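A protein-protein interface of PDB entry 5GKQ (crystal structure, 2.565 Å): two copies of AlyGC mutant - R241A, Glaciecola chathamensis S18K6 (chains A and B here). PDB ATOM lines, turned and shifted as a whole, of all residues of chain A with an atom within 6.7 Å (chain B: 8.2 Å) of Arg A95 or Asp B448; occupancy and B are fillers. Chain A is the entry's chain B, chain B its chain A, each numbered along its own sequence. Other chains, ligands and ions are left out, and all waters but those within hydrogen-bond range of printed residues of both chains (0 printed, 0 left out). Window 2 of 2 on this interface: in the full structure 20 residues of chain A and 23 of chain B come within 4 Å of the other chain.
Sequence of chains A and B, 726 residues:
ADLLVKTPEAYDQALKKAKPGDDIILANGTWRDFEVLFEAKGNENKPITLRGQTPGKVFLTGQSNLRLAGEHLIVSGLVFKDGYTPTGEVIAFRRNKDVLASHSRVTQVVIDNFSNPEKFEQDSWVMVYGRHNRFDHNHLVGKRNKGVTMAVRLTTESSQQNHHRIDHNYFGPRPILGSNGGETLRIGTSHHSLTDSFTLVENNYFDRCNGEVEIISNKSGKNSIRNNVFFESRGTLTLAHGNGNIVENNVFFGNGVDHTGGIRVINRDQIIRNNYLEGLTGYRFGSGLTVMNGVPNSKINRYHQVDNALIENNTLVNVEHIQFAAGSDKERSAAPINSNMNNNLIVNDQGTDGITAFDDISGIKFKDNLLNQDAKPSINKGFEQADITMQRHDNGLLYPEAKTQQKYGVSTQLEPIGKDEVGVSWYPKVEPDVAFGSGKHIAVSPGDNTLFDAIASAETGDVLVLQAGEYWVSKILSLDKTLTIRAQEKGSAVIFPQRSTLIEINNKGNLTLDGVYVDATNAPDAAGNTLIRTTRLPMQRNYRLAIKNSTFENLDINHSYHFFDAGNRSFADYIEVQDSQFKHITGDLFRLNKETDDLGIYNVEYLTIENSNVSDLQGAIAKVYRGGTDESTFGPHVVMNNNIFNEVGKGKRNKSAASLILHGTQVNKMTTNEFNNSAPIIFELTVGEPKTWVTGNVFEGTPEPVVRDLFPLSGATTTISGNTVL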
ATOM      1  N   LEU A  37      26.705 -12.012  -8.575  1.00  0.00           N
ATOM      2  CA  LEU A  37      25.424 -11.453  -8.974  1.00  0.00           C
ATOM      3  C   LEU A  37      24.399 -11.919  -7.955  1.00  0.00           C
ATOM      4  O   LEU A  37      23.918 -13.051  -8.023  1.00  0.00           O
ATOM      5  CB  LEU A  37      25.030 -11.881 -10.377  1.00  0.00           C
ATOM      6  CG  LEU A  37      23.609 -11.406 -10.693  1.00  0.00           C
ATOM      7  CD1 LEU A  37      23.463  -9.908 -10.489  1.00  0.00           C
ATOM      8  CD2 LEU A  37      23.229 -11.801 -12.091  1.00  0.00           C
ATOM      9  N   GLU A  39      20.960 -11.614  -7.023  1.00  0.00           N
ATOM     10  CA  GLU A  39      19.694 -11.209  -7.634  1.00  0.00           C
ATOM     11  C   GLU A  39      18.551 -11.983  -6.994  1.00  0.00           C
ATOM     12  O   GLU A  39      18.393 -13.181  -7.239  1.00  0.00           O
ATOM     13  CB  GLU A  39      19.722 -11.450  -9.141  1.00  0.00           C
ATOM     14  CG  GLU A  39      18.417 -11.100  -9.829  1.00  0.00           C
ATOM     15  CD  GLU A  39      18.493 -11.112 -11.350  1.00  0.00           C
ATOM     16  OE1 GLU A  39      17.629 -10.469 -11.974  1.00  0.00           O
ATOM     17  OE2 GLU A  39      19.388 -11.769 -11.919  1.00  0.00           O
ATOM     18  N   ARG A  67      27.133  -7.265  -7.678  1.00  0.00           N
ATOM     19  CA  ARG A  67      25.971  -6.613  -8.268  1.00  0.00           C
ATOM     20  C   ARG A  67      24.723  -7.096  -7.557  1.00  0.00           C
ATOM     21  O   ARG A  67      24.445  -8.298  -7.533  1.00  0.00           O
ATOM     22  CB  ARG A  67      25.841  -6.898  -9.775  1.00  0.00           C
ATOM     23  CG  ARG A  67      27.056  -6.562 -10.622  1.00  0.00           C
ATOM     24  CD  ARG A  67      26.882  -6.978 -12.066  1.00  0.00           C
ATOM     25  NE  ARG A  67      27.088  -8.409 -12.296  1.00  0.00           N
ATOM     26  CZ  ARG A  67      26.563  -9.068 -13.324  1.00  0.00           C
ATOM     27  NH1 ARG A  67      25.812  -8.432 -14.199  1.00  0.00           N
ATOM     28  NH2 ARG A  67      26.777 -10.347 -13.492  1.00  0.00           N
ATOM     29  N   LEU A  68      23.976  -6.161  -6.991  1.00  0.00           N
ATOM     30  CA  LEU A  68      22.679  -6.443  -6.403  1.00  0.00           C
ATOM     31  C   LEU A  68      21.592  -6.171  -7.429  1.00  0.00           C
ATOM     32  O   LEU A  68      21.727  -5.279  -8.266  1.00  0.00           O
ATOM     33  CB  LEU A  68      22.422  -5.578  -5.172  1.00  0.00           C
ATOM     34  CG  LEU A  68      23.384  -5.629  -3.990  1.00  0.00           C
ATOM     35  CD1 LEU A  68      24.601  -4.763  -4.274  1.00  0.00           C
ATOM     36  CD2 LEU A  68      22.660  -5.177  -2.728  1.00  0.00           C
ATOM     37  N   ALA A  69      20.498  -6.922  -7.342  1.00  0.00           N
ATOM     38  CA  ALA A  69      19.392  -6.798  -8.283  1.00  0.00           C
ATOM     39  C   ALA A  69      18.176  -7.444  -7.654  1.00  0.00           C
ATOM     40  O   ALA A  69      18.293  -8.487  -7.023  1.00  0.00           O
ATOM     41  CB  ALA A  69      19.699  -7.461  -9.625  1.00  0.00           C
ATOM     42  N   GLY A  70      17.015  -6.831  -7.837  1.00  0.00           N
ATOM     43  CA  GLY A  70      15.841  -7.233  -7.100  1.00  0.00           C
ATOM     44  C   GLY A  70      15.504  -6.212  -6.041  1.00  0.00           C
ATOM     45  O   GLY A  70      15.796  -5.029  -6.205  1.00  0.00           O
ATOM     46  N   ALA A  92      27.856  -2.539  -7.623  1.00  0.00           N
ATOM     47  CA  ALA A  92      26.812  -1.902  -8.404  1.00  0.00           C
ATOM     48  C   ALA A  92      25.457  -2.328  -7.877  1.00  0.00           C
ATOM     49  O   ALA A  92      25.227  -3.515  -7.647  1.00  0.00           O
ATOM     50  CB  ALA A  92      26.902  -2.281  -9.870  1.00  0.00           C
ATOM     51  N   PHE A  93      24.550  -1.368  -7.731  1.00  0.00           N
ATOM     52  CA  PHE A  93      23.181  -1.640  -7.301  1.00  0.00           C
ATOM     53  C   PHE A  93      22.265  -1.953  -8.476  1.00  0.00           C
ATOM     54  O   PHE A  93      21.157  -1.429  -8.554  1.00  0.00           O
ATOM     55  CB  PHE A  93      22.630  -0.467  -6.509  1.00  0.00           C
ATOM     56  CG  PHE A  93      23.057  -0.432  -5.079  1.00  0.00           C
ATOM     57  CD1 PHE A  93      24.294   0.064  -4.723  1.00  0.00           C
ATOM     58  CD2 PHE A  93      22.217  -0.868  -4.083  1.00  0.00           C
ATOM     59  CE1 PHE A  93      24.682   0.118  -3.415  1.00  0.00           C
ATOM     60  CE2 PHE A  93      22.610  -0.819  -2.763  1.00  0.00           C
ATOM     61  CZ  PHE A  93      23.846  -0.318  -2.431  1.00  0.00           C
ATOM     62  N   ARG A  94      22.708  -2.816  -9.386  1.00  0.00           N
ATOM     63  CA  ARG A  94      21.881  -3.265 -10.501  1.00  0.00           C
ATOM     64  C   ARG A  94      22.527  -4.496 -11.125  1.00  0.00           C
ATOM     65  O   ARG A  94      23.730  -4.716 -10.990  1.00  0.00           O
ATOM     66  CB  ARG A  94      21.715  -2.173 -11.551  1.00  0.00           C
ATOM     67  CG  ARG A  94      22.927  -2.027 -12.425  1.00  0.00           C
ATOM     68  CD  ARG A  94      22.784  -0.960 -13.468  1.00  0.00           C
ATOM     69  NE  ARG A  94      23.898  -1.045 -14.387  1.00  0.00           N
ATOM     70  CZ  ARG A  94      23.987  -0.351 -15.510  1.00  0.00           C
ATOM     71  NH1 ARG A  94      25.039  -0.495 -16.291  1.00  0.00           N
ATOM     72  NH2 ARG A  94      23.026   0.494 -15.848  1.00  0.00           N
ATOM     73  N   ARG A  95      21.719  -5.306 -11.802  1.00  0.00           N
ATOM     74  CA  ARG A  95      22.309  -6.362 -12.613  1.00  0.00           C
ATOM     75  C   ARG A  95      22.891  -5.780 -13.880  1.00  0.00           C
ATOM     76  O   ARG A  95      24.034  -6.071 -14.247  1.00  0.00           O
ATOM     77  CB  ARG A  95      21.271  -7.423 -12.964  1.00  0.00           C
ATOM     78  CG  ARG A  95      21.659  -8.289 -14.153  1.00  0.00           C
ATOM     79  CD  ARG A  95      20.882  -9.589 -14.170  1.00  0.00           C
ATOM     80  NE  ARG A  95      21.432 -10.546 -15.131  1.00  0.00           N
ATOM     81  CZ  ARG A  95      21.143 -11.849 -15.158  1.00  0.00           C
ATOM     82  NH1 ARG A  95      20.307 -12.374 -14.268  1.00  0.00           N
ATOM     83  NH2 ARG A  95      21.696 -12.628 -16.078  1.00  0.00           N
ATOM     84  N   ASN A  96      22.104  -4.943 -14.533  1.00  0.00           N
ATOM     85  CA  ASN A  96      22.389  -4.259 -15.783  1.00  0.00           C
ATOM     86  C   ASN A  96      21.272  -3.232 -15.949  1.00  0.00           C
ATOM     87  O   ASN A  96      20.523  -2.959 -15.006  1.00  0.00           O
ATOM     88  CB  ASN A  96      22.492  -5.247 -16.943  1.00  0.00           C
ATOM     89  CG  ASN A  96      21.253  -6.087 -17.091  1.00  0.00           C
ATOM     90  OD1 ASN A  96      20.139  -5.599 -16.938  1.00  0.00           O
ATOM     91  ND2 ASN A  96      21.438  -7.359 -17.403  1.00  0.00           N
ATOM     92  N   LYS A  97      21.145  -2.659 -17.143  1.00  0.00           N
ATOM     93  CA  LYS A  97      20.131  -1.634 -17.354  1.00  0.00           C
ATOM     94  C   LYS A  97      18.714  -2.179 -17.229  1.00  0.00           C
ATOM     95  O   LYS A  97      17.789  -1.402 -17.005  1.00  0.00           O
ATOM     96  CB  LYS A  97      20.307  -0.997 -18.728  1.00  0.00           C
ATOM     97  CG  LYS A  97      19.715  -1.834 -19.828  1.00  0.00           C
ATOM     98  CD  LYS A  97      20.393  -1.589 -21.158  1.00  0.00           C
ATOM     99  CE  LYS A  97      19.765  -2.453 -22.245  1.00  0.00           C
ATOM    100  NZ  LYS A  97      18.358  -2.021 -22.516  1.00  0.00           N
ATOM    101  N   ASP A  98      18.528  -3.489 -17.350  1.00  0.00           N
ATOM    102  CA  ASP A  98      17.192  -4.077 -17.344  1.00  0.00           C
ATOM    103  C   ASP A  98      16.684  -4.455 -15.958  1.00  0.00           C
ATOM    104  O   ASP A  98      15.472  -4.416 -15.736  1.00  0.00           O
ATOM    105  CB  ASP A  98      17.143  -5.324 -18.235  1.00  0.00           C
ATOM    106  CG  ASP A  98      17.624  -5.060 -19.657  1.00  0.00           C
ATOM    107  OD1 ASP A  98      17.446  -3.924 -20.162  1.00  0.00           O
ATOM    108  OD2 ASP A  98      18.159  -6.005 -20.277  1.00  0.00           O
ATOM    109  N   VAL A  99      17.554  -4.827 -15.019  1.00  0.00           N
ATOM    110  CA  VAL A  99      17.142  -5.193 -13.666  1.00  0.00           C
ATOM    111  C   VAL A  99      17.927  -4.349 -12.680  1.00  0.00           C
ATOM    112  O   VAL A  99      19.128  -4.555 -12.507  1.00  0.00           O
ATOM    113  CB  VAL A  99      17.358  -6.677 -13.370  1.00  0.00           C
ATOM    114  CG1 VAL A  99      16.699  -7.033 -12.068  1.00  0.00           C
ATOM    115  CG2 VAL A  99      16.820  -7.509 -14.484  1.00  0.00           C
ATOM    116  N   LEU A 100      17.262  -3.418 -12.025  1.00  0.00           N
ATOM    117  CA  LEU A 100      17.936  -2.631 -11.014  1.00  0.00           C
ATOM    118  C   LEU A 100      17.709  -3.258  -9.646  1.00  0.00           C
ATOM    119  O   LEU A 100      16.988  -4.241  -9.495  1.00  0.00           O
ATOM    120  CB  LEU A 100      17.439  -1.190 -11.026  1.00  0.00           C
ATOM    121  CG  LEU A 100      17.371  -0.407 -12.342  1.00  0.00           C
ATOM    122  CD1 LEU A 100      16.956   1.018 -12.039  1.00  0.00           C
ATOM    123  CD2 LEU A 100      18.680  -0.443 -13.074  1.00  0.00           C
ATOM    124  N   ALA A 101      18.320  -2.675  -8.631  1.00  0.00           N
ATOM    125  CA  ALA A 101      18.033  -3.034  -7.258  1.00  0.00           C
ATOM    126  C   ALA A 101      17.485  -1.821  -6.540  1.00  0.00           C
ATOM    127  O   ALA A 101      18.009  -0.715  -6.680  1.00  0.00           O
ATOM    128  CB  ALA A 101      19.278  -3.544  -6.514  1.00  0.00           C
ATOM    129  N   SER B 445      25.188 -14.862 -28.834  1.00  0.00           N
ATOM    130  CA  SER B 445      23.911 -14.190 -28.677  1.00  0.00           C
ATOM    131  C   SER B 445      24.062 -13.068 -27.668  1.00  0.00           C
ATOM    132  O   SER B 445      25.003 -13.066 -26.874  1.00  0.00           O
ATOM    133  CB  SER B 445      22.820 -15.169 -28.225  1.00  0.00           C
ATOM    134  OG  SER B 445      22.313 -15.880 -29.337  1.00  0.00           O
ATOM    135  N   PRO B 446      23.173 -12.076 -27.696  1.00  0.00           N
ATOM    136  CA  PRO B 446      23.191 -10.982 -26.718  1.00  0.00           C
ATOM    137  C   PRO B 446      22.667 -11.417 -25.360  1.00  0.00           C
ATOM    138  O   PRO B 446      21.923 -12.396 -25.350  1.00  0.00           O
ATOM    139  CB  PRO B 446      22.271  -9.954 -27.349  1.00  0.00           C
ATOM    140  CG  PRO B 446      21.406 -10.724 -28.253  1.00  0.00           C
ATOM    141  CD  PRO B 446      22.244 -11.810 -28.797  1.00  0.00           C
ATOM    142  N   GLY B 447      23.036 -10.762 -24.251  1.00  0.00           N
ATOM    143  CA  GLY B 447      23.947  -9.624 -24.209  1.00  0.00           C
ATOM    144  C   GLY B 447      24.707  -9.381 -22.897  1.00  0.00           C
ATOM    145  O   GLY B 447      25.456  -8.401 -22.793  1.00  0.00           O
ATOM    146  N   ASP B 448      24.547 -10.271 -21.906  1.00  0.00           N
ATOM    147  CA  ASP B 448      25.096 -10.071 -20.553  1.00  0.00           C
ATOM    148  C   ASP B 448      26.585 -10.409 -20.558  1.00  0.00           C
ATOM    149  O   ASP B 448      27.016 -11.492 -20.137  1.00  0.00           O
ATOM    150  CB  ASP B 448      24.334 -10.914 -19.525  1.00  0.00           C
ATOM    151  CG  ASP B 448      24.355 -10.309 -18.105  1.00  0.00           C
ATOM    152  OD1 ASP B 448      23.677  -9.286 -17.867  1.00  0.00           O
ATOM    153  OD2 ASP B 448      25.031 -10.868 -17.215  1.00  0.00           O
ATOM    154  N   ASN B 449      27.383  -9.440 -21.017  1.00  0.00           N
ATOM    155  CA  ASN B 449      28.815  -9.636 -21.274  1.00  0.00           C
ATOM    156  C   ASN B 449      29.050 -10.940 -22.026  1.00  0.00           C
ATOM    157  O   ASN B 449      29.823 -11.811 -21.637  1.00  0.00           O
ATOM    158  CB  ASN B 449      29.617  -9.551 -19.987  1.00  0.00           C
ATOM    159  CG  ASN B 449      29.815  -8.121 -19.562  1.00  0.00           C
ATOM    160  OD1 ASN B 449      29.829  -7.801 -18.379  1.00  0.00           O
ATOM    161  ND2 ASN B 449      29.937  -7.244 -20.532  1.00  0.00           N
ATOM    162  N   THR B 450      28.332 -11.055 -23.139  1.00  0.00           N
ATOM    163  CA  THR B 450      28.285 -12.281 -23.919  1.00  0.00           C
ATOM    164  C   THR B 450      29.479 -12.373 -24.841  1.00  0.00           C
ATOM    165  O   THR B 450      29.996 -13.468 -25.098  1.00  0.00           O
ATOM    166  CB  THR B 450      26.994 -12.307 -24.729  1.00  0.00           C
ATOM    167  OG1 THR B 450      26.731 -10.985 -25.208  1.00  0.00           O
ATOM    168  CG2 THR B 450      25.822 -12.749 -23.869  1.00  0.00           C
ATOM    169  N   LEU B 451      29.917 -11.222 -25.346  1.00  0.00           N
ATOM    170  CA  LEU B 451      31.024 -11.175 -26.285  1.00  0.00           C
ATOM    171  C   LEU B 451      32.338 -11.426 -25.574  1.00  0.00           C
ATOM    172  O   LEU B 451      33.227 -12.084 -26.114  1.00  0.00           O
ATOM    173  CB  LEU B 451      31.033  -9.815 -26.990  1.00  0.00           C
ATOM    174  CG  LEU B 451      31.938  -9.551 -28.194  1.00  0.00           C
ATOM    175  CD1 LEU B 451      31.644 -10.509 -29.323  1.00  0.00           C
ATOM    176  CD2 LEU B 451      31.708  -8.167 -28.655  1.00  0.00           C
ATOM    177  N   PHE B 452      32.475 -10.895 -24.361  1.00  0.00           N
ATOM    178  CA  PHE B 452      33.675 -11.125 -23.570  1.00  0.00           C
ATOM    179  C   PHE B 452      33.891 -12.612 -23.346  1.00  0.00           C
ATOM    180  O   PHE B 452      35.005 -13.123 -23.500  1.00  0.00           O
ATOM    181  CB  PHE B 452      33.557 -10.390 -22.236  1.00  0.00           C
ATOM    182  CG  PHE B 452      34.649 -10.705 -21.274  1.00  0.00           C
ATOM    183  CD1 PHE B 452      34.545 -11.793 -20.417  1.00  0.00           C
ATOM    184  CD2 PHE B 452      35.778  -9.916 -21.209  1.00  0.00           C
ATOM    185  CE1 PHE B 452      35.550 -12.097 -19.526  1.00  0.00           C
ATOM    186  CE2 PHE B 452      36.792 -10.208 -20.305  1.00  0.00           C
ATOM    187  CZ  PHE B 452      36.680 -11.298 -19.470  1.00  0.00           C
ATOM    188  N   ASP B 453      32.827 -13.320 -22.982  1.00  0.00           N
ATOM    189  CA  ASP B 453      32.947 -14.742 -22.693  1.00  0.00           C
ATOM    190  C   ASP B 453      33.216 -15.543 -23.956  1.00  0.00           C
ATOM    191  O   ASP B 453      34.009 -16.491 -23.938  1.00  0.00           O
ATOM    192  CB  ASP B 453      31.689 -15.223 -21.986  1.00  0.00           C
ATOM    193  CG  ASP B 453      31.591 -14.688 -20.583  1.00  0.00           C
ATOM    194  OD1 ASP B 453      32.604 -14.767 -19.855  1.00  0.00           O
ATOM    195  OD2 ASP B 453      30.520 -14.167 -20.217  1.00  0.00           O
ATOM    196  N   GLU B 470      21.491  -6.436 -29.313  1.00  0.00           N
ATOM    197  CA  GLU B 470      22.394  -5.485 -28.688  1.00  0.00           C
ATOM    198  C   GLU B 470      23.382  -6.208 -27.788  1.00  0.00           C
ATOM    199  O   GLU B 470      23.013  -7.104 -27.030  1.00  0.00           O
ATOM    200  CB  GLU B 470      21.611  -4.458 -27.886  1.00  0.00           C
ATOM    201  CG  GLU B 470      20.470  -3.850 -28.662  1.00  0.00           C
ATOM    202  CD  GLU B 470      19.716  -2.840 -27.862  1.00  0.00           C
ATOM    203  OE1 GLU B 470      19.948  -2.778 -26.648  1.00  0.00           O
ATOM    204  OE2 GLU B 470      18.886  -2.111 -28.427  1.00  0.00           O
ATOM    205  N   TYR B 471      24.641  -5.810 -27.875  1.00  0.00           N
ATOM    206  CA  TYR B 471      25.729  -6.418 -27.111  1.00  0.00           C
ATOM    207  C   TYR B 471      26.290  -5.362 -26.171  1.00  0.00           C
ATOM    208  O   TYR B 471      27.160  -4.583 -26.553  1.00  0.00           O
ATOM    209  CB  TYR B 471      26.805  -6.967 -28.041  1.00  0.00           C
ATOM    210  CG  TYR B 471      26.356  -8.191 -28.793  1.00  0.00           C
ATOM    211  CD1 TYR B 471      25.546  -8.083 -29.908  1.00  0.00           C
ATOM    212  CD2 TYR B 471      26.730  -9.458 -28.376  1.00  0.00           C
ATOM    213  CE1 TYR B 471      25.120  -9.198 -30.594  1.00  0.00           C
ATOM    214  CE2 TYR B 471      26.310 -10.586 -29.057  1.00  0.00           C
ATOM    215  CZ  TYR B 471      25.505 -10.453 -30.165  1.00  0.00           C
ATOM    216  OH  TYR B 471      25.096 -11.584 -30.843  1.00  0.00           O
ATOM    217  N   TRP B 472      25.798  -5.333 -24.945  1.00  0.00           N
ATOM    218  CA  TRP B 472      26.307  -4.382 -23.976  1.00  0.00           C
ATOM    219  C   TRP B 472      27.564  -4.946 -23.342  1.00  0.00           C
ATOM    220  O   TRP B 472      27.583  -6.086 -22.886  1.00  0.00           O
ATOM    221  CB  TRP B 472      25.241  -4.072 -22.932  1.00  0.00           C
ATOM    222  CG  TRP B 472      24.061  -3.360 -23.543  1.00  0.00           C
ATOM    223  CD1 TRP B 472      23.045  -3.926 -24.241  1.00  0.00           C
ATOM    224  CD2 TRP B 472      23.806  -1.954 -23.534  1.00  0.00           C
ATOM    225  NE1 TRP B 472      22.158  -2.969 -24.645  1.00  0.00           N
ATOM    226  CE2 TRP B 472      22.605  -1.747 -24.227  1.00  0.00           C
ATOM    227  CE3 TRP B 472      24.468  -0.852 -22.993  1.00  0.00           C
ATOM    228  CZ2 TRP B 472      22.056  -0.480 -24.408  1.00  0.00           C
ATOM    229  CZ3 TRP B 472      23.917   0.406 -23.168  1.00  0.00           C
ATOM    230  CH2 TRP B 472      22.726   0.580 -23.874  1.00  0.00           C
ATOM    231  N   VAL B 473      28.619  -4.150 -23.334  1.00  0.00           N
ATOM    232  CA  VAL B 473      29.957  -4.616 -23.038  1.00  0.00           C
ATOM    233  C   VAL B 473      30.503  -3.778 -21.894  1.00  0.00           C
ATOM    234  O   VAL B 473      30.896  -2.623 -22.095  1.00  0.00           O
ATOM    235  CB  VAL B 473      30.850  -4.529 -24.274  1.00  0.00           C
ATOM    236  CG1 VAL B 473      32.269  -4.869 -23.934  1.00  0.00           C
ATOM    237  CG2 VAL B 473      30.308  -5.453 -25.344  1.00  0.00           C
ATOM    238  N   SER B 474      30.546  -4.365 -20.699  1.00  0.00           N
ATOM    239  CA  SER B 474      31.030  -3.703 -19.496  1.00  0.00           C
ATOM    240  C   SER B 474      32.451  -4.101 -19.121  1.00  0.00           C
ATOM    241  O   SER B 474      32.996  -3.556 -18.162  1.00  0.00           O
ATOM    242  CB  SER B 474      30.090  -3.995 -18.332  1.00  0.00           C
ATOM    243  OG  SER B 474      29.919  -5.389 -18.190  1.00  0.00           O
ATOM    244  N   LYS B 475      33.059  -5.030 -19.844  1.00  0.00           N
ATOM    245  CA  LYS B 475      34.431  -5.453 -19.610  1.00  0.00           C
ATOM    246  C   LYS B 475      35.258  -5.103 -20.830  1.00  0.00           C
ATOM    247  O   LYS B 475      34.736  -5.016 -21.936  1.00  0.00           O
ATOM    248  CB  LYS B 475      34.542  -6.967 -19.356  1.00  0.00           C
ATOM    249  CG  LYS B 475      33.814  -7.466 -18.133  1.00  0.00           C
ATOM    250  CD  LYS B 475      33.796  -8.993 -18.078  1.00  0.00           C
ATOM    251  CE  LYS B 475      33.237  -9.501 -16.763  1.00  0.00           C
ATOM    252  NZ  LYS B 475      33.464 -10.961 -16.629  1.00  0.00           N
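N of Val A99 sits at hydrogen-bond distance from OD1 of Asn A96 (3.3 Å).
OD1 of Asp A98 lies within salt-bridge range of NZ of Lys A97, 3.2 Å away.
The side-chain carboxylate of Glu A39 is in salt-bridge range of the guanidinium group of Arg A95.
NE1 of Trp B472 is in hydrogen-bond range of OE1 of Glu B470.
The guanidinium group (NH1) of Arg A67 lies within hydrogen-bond range of the backbone carbonyl oxygen (O) of Arg A95 (3.0 Å).
The side-chain amide oxygen of Asn A96 lies within hydrogen-bond range of the backbone NH of Asp A98 (2.7 Å).
Of the printed residues of chain B, Arg A67 touches Asp B448.
Of chain B, only Asp B448 (3.8 Å) comes within 4 Å of Arg A95.
Of the printed residues of chain B, Asn A96 touches Asp B448.
Of the printed residues of chain B, Lys A97 touches Trp B472.
Asp B448 touches three residues of chain A.
Leu B451 touches none of the printed residues of chain A.
Printed residues of chain A within 4 Å of Trp B472: Lys A97 (3.4 Å).
Lys B475 touches none of the printed residues of chain A.
The nearest residue of chain B that does not touch Arg A95 is Ser B474 (7.1 Å).
The nearest residue of chain A that does not touch Asp B448 is Leu A37 (5.5 Å).
The nearest printed residue of chain B that does not touch Arg A67 is Asn B449 (5.8 Å).
The side-chain carboxylate (OD2) of Asp B448 is in salt-bridge range of the guanidinium group (NH1) of Arg A67 (3.95 Å).
The side-chain carboxylate (OD1) of Asp B448 lies within salt-bridge range of the guanidinium group (NE) of Arg A95, at 3.8 Å.
The side-chain carboxylate of Asp B448 is in hydrogen-bond range of the side-chain amide nitrogen of Asn A96 (3.0 Å).
Of the 15 printed residues of chain B, 2 touch a printed residue of chain A.
Hydrophobic or aromatic side chains of chain B that line the printed part of chain A: Trp B472.
Along chain B the printed residues that touch a printed residue of chain A span positions 448 to 472.
Among the printed residues, 4 pairs touch across the chains.
Among the printed residues, Asp or Glu carboxylates within 4 Å of a Lys or Arg side-chain nitrogen of the other chain: Arg A67 with Asp B448 (3.95 Å) and Arg A95 with Asp B448 (3.8 Å).
Lys A97 touches Trp B472 (CE to NE1, 3.4 Å).
No position is printed for both chains.
Of the 4 pairs that touch across the chains among the printed residues, none has its exchanged pair printed and touching as well.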
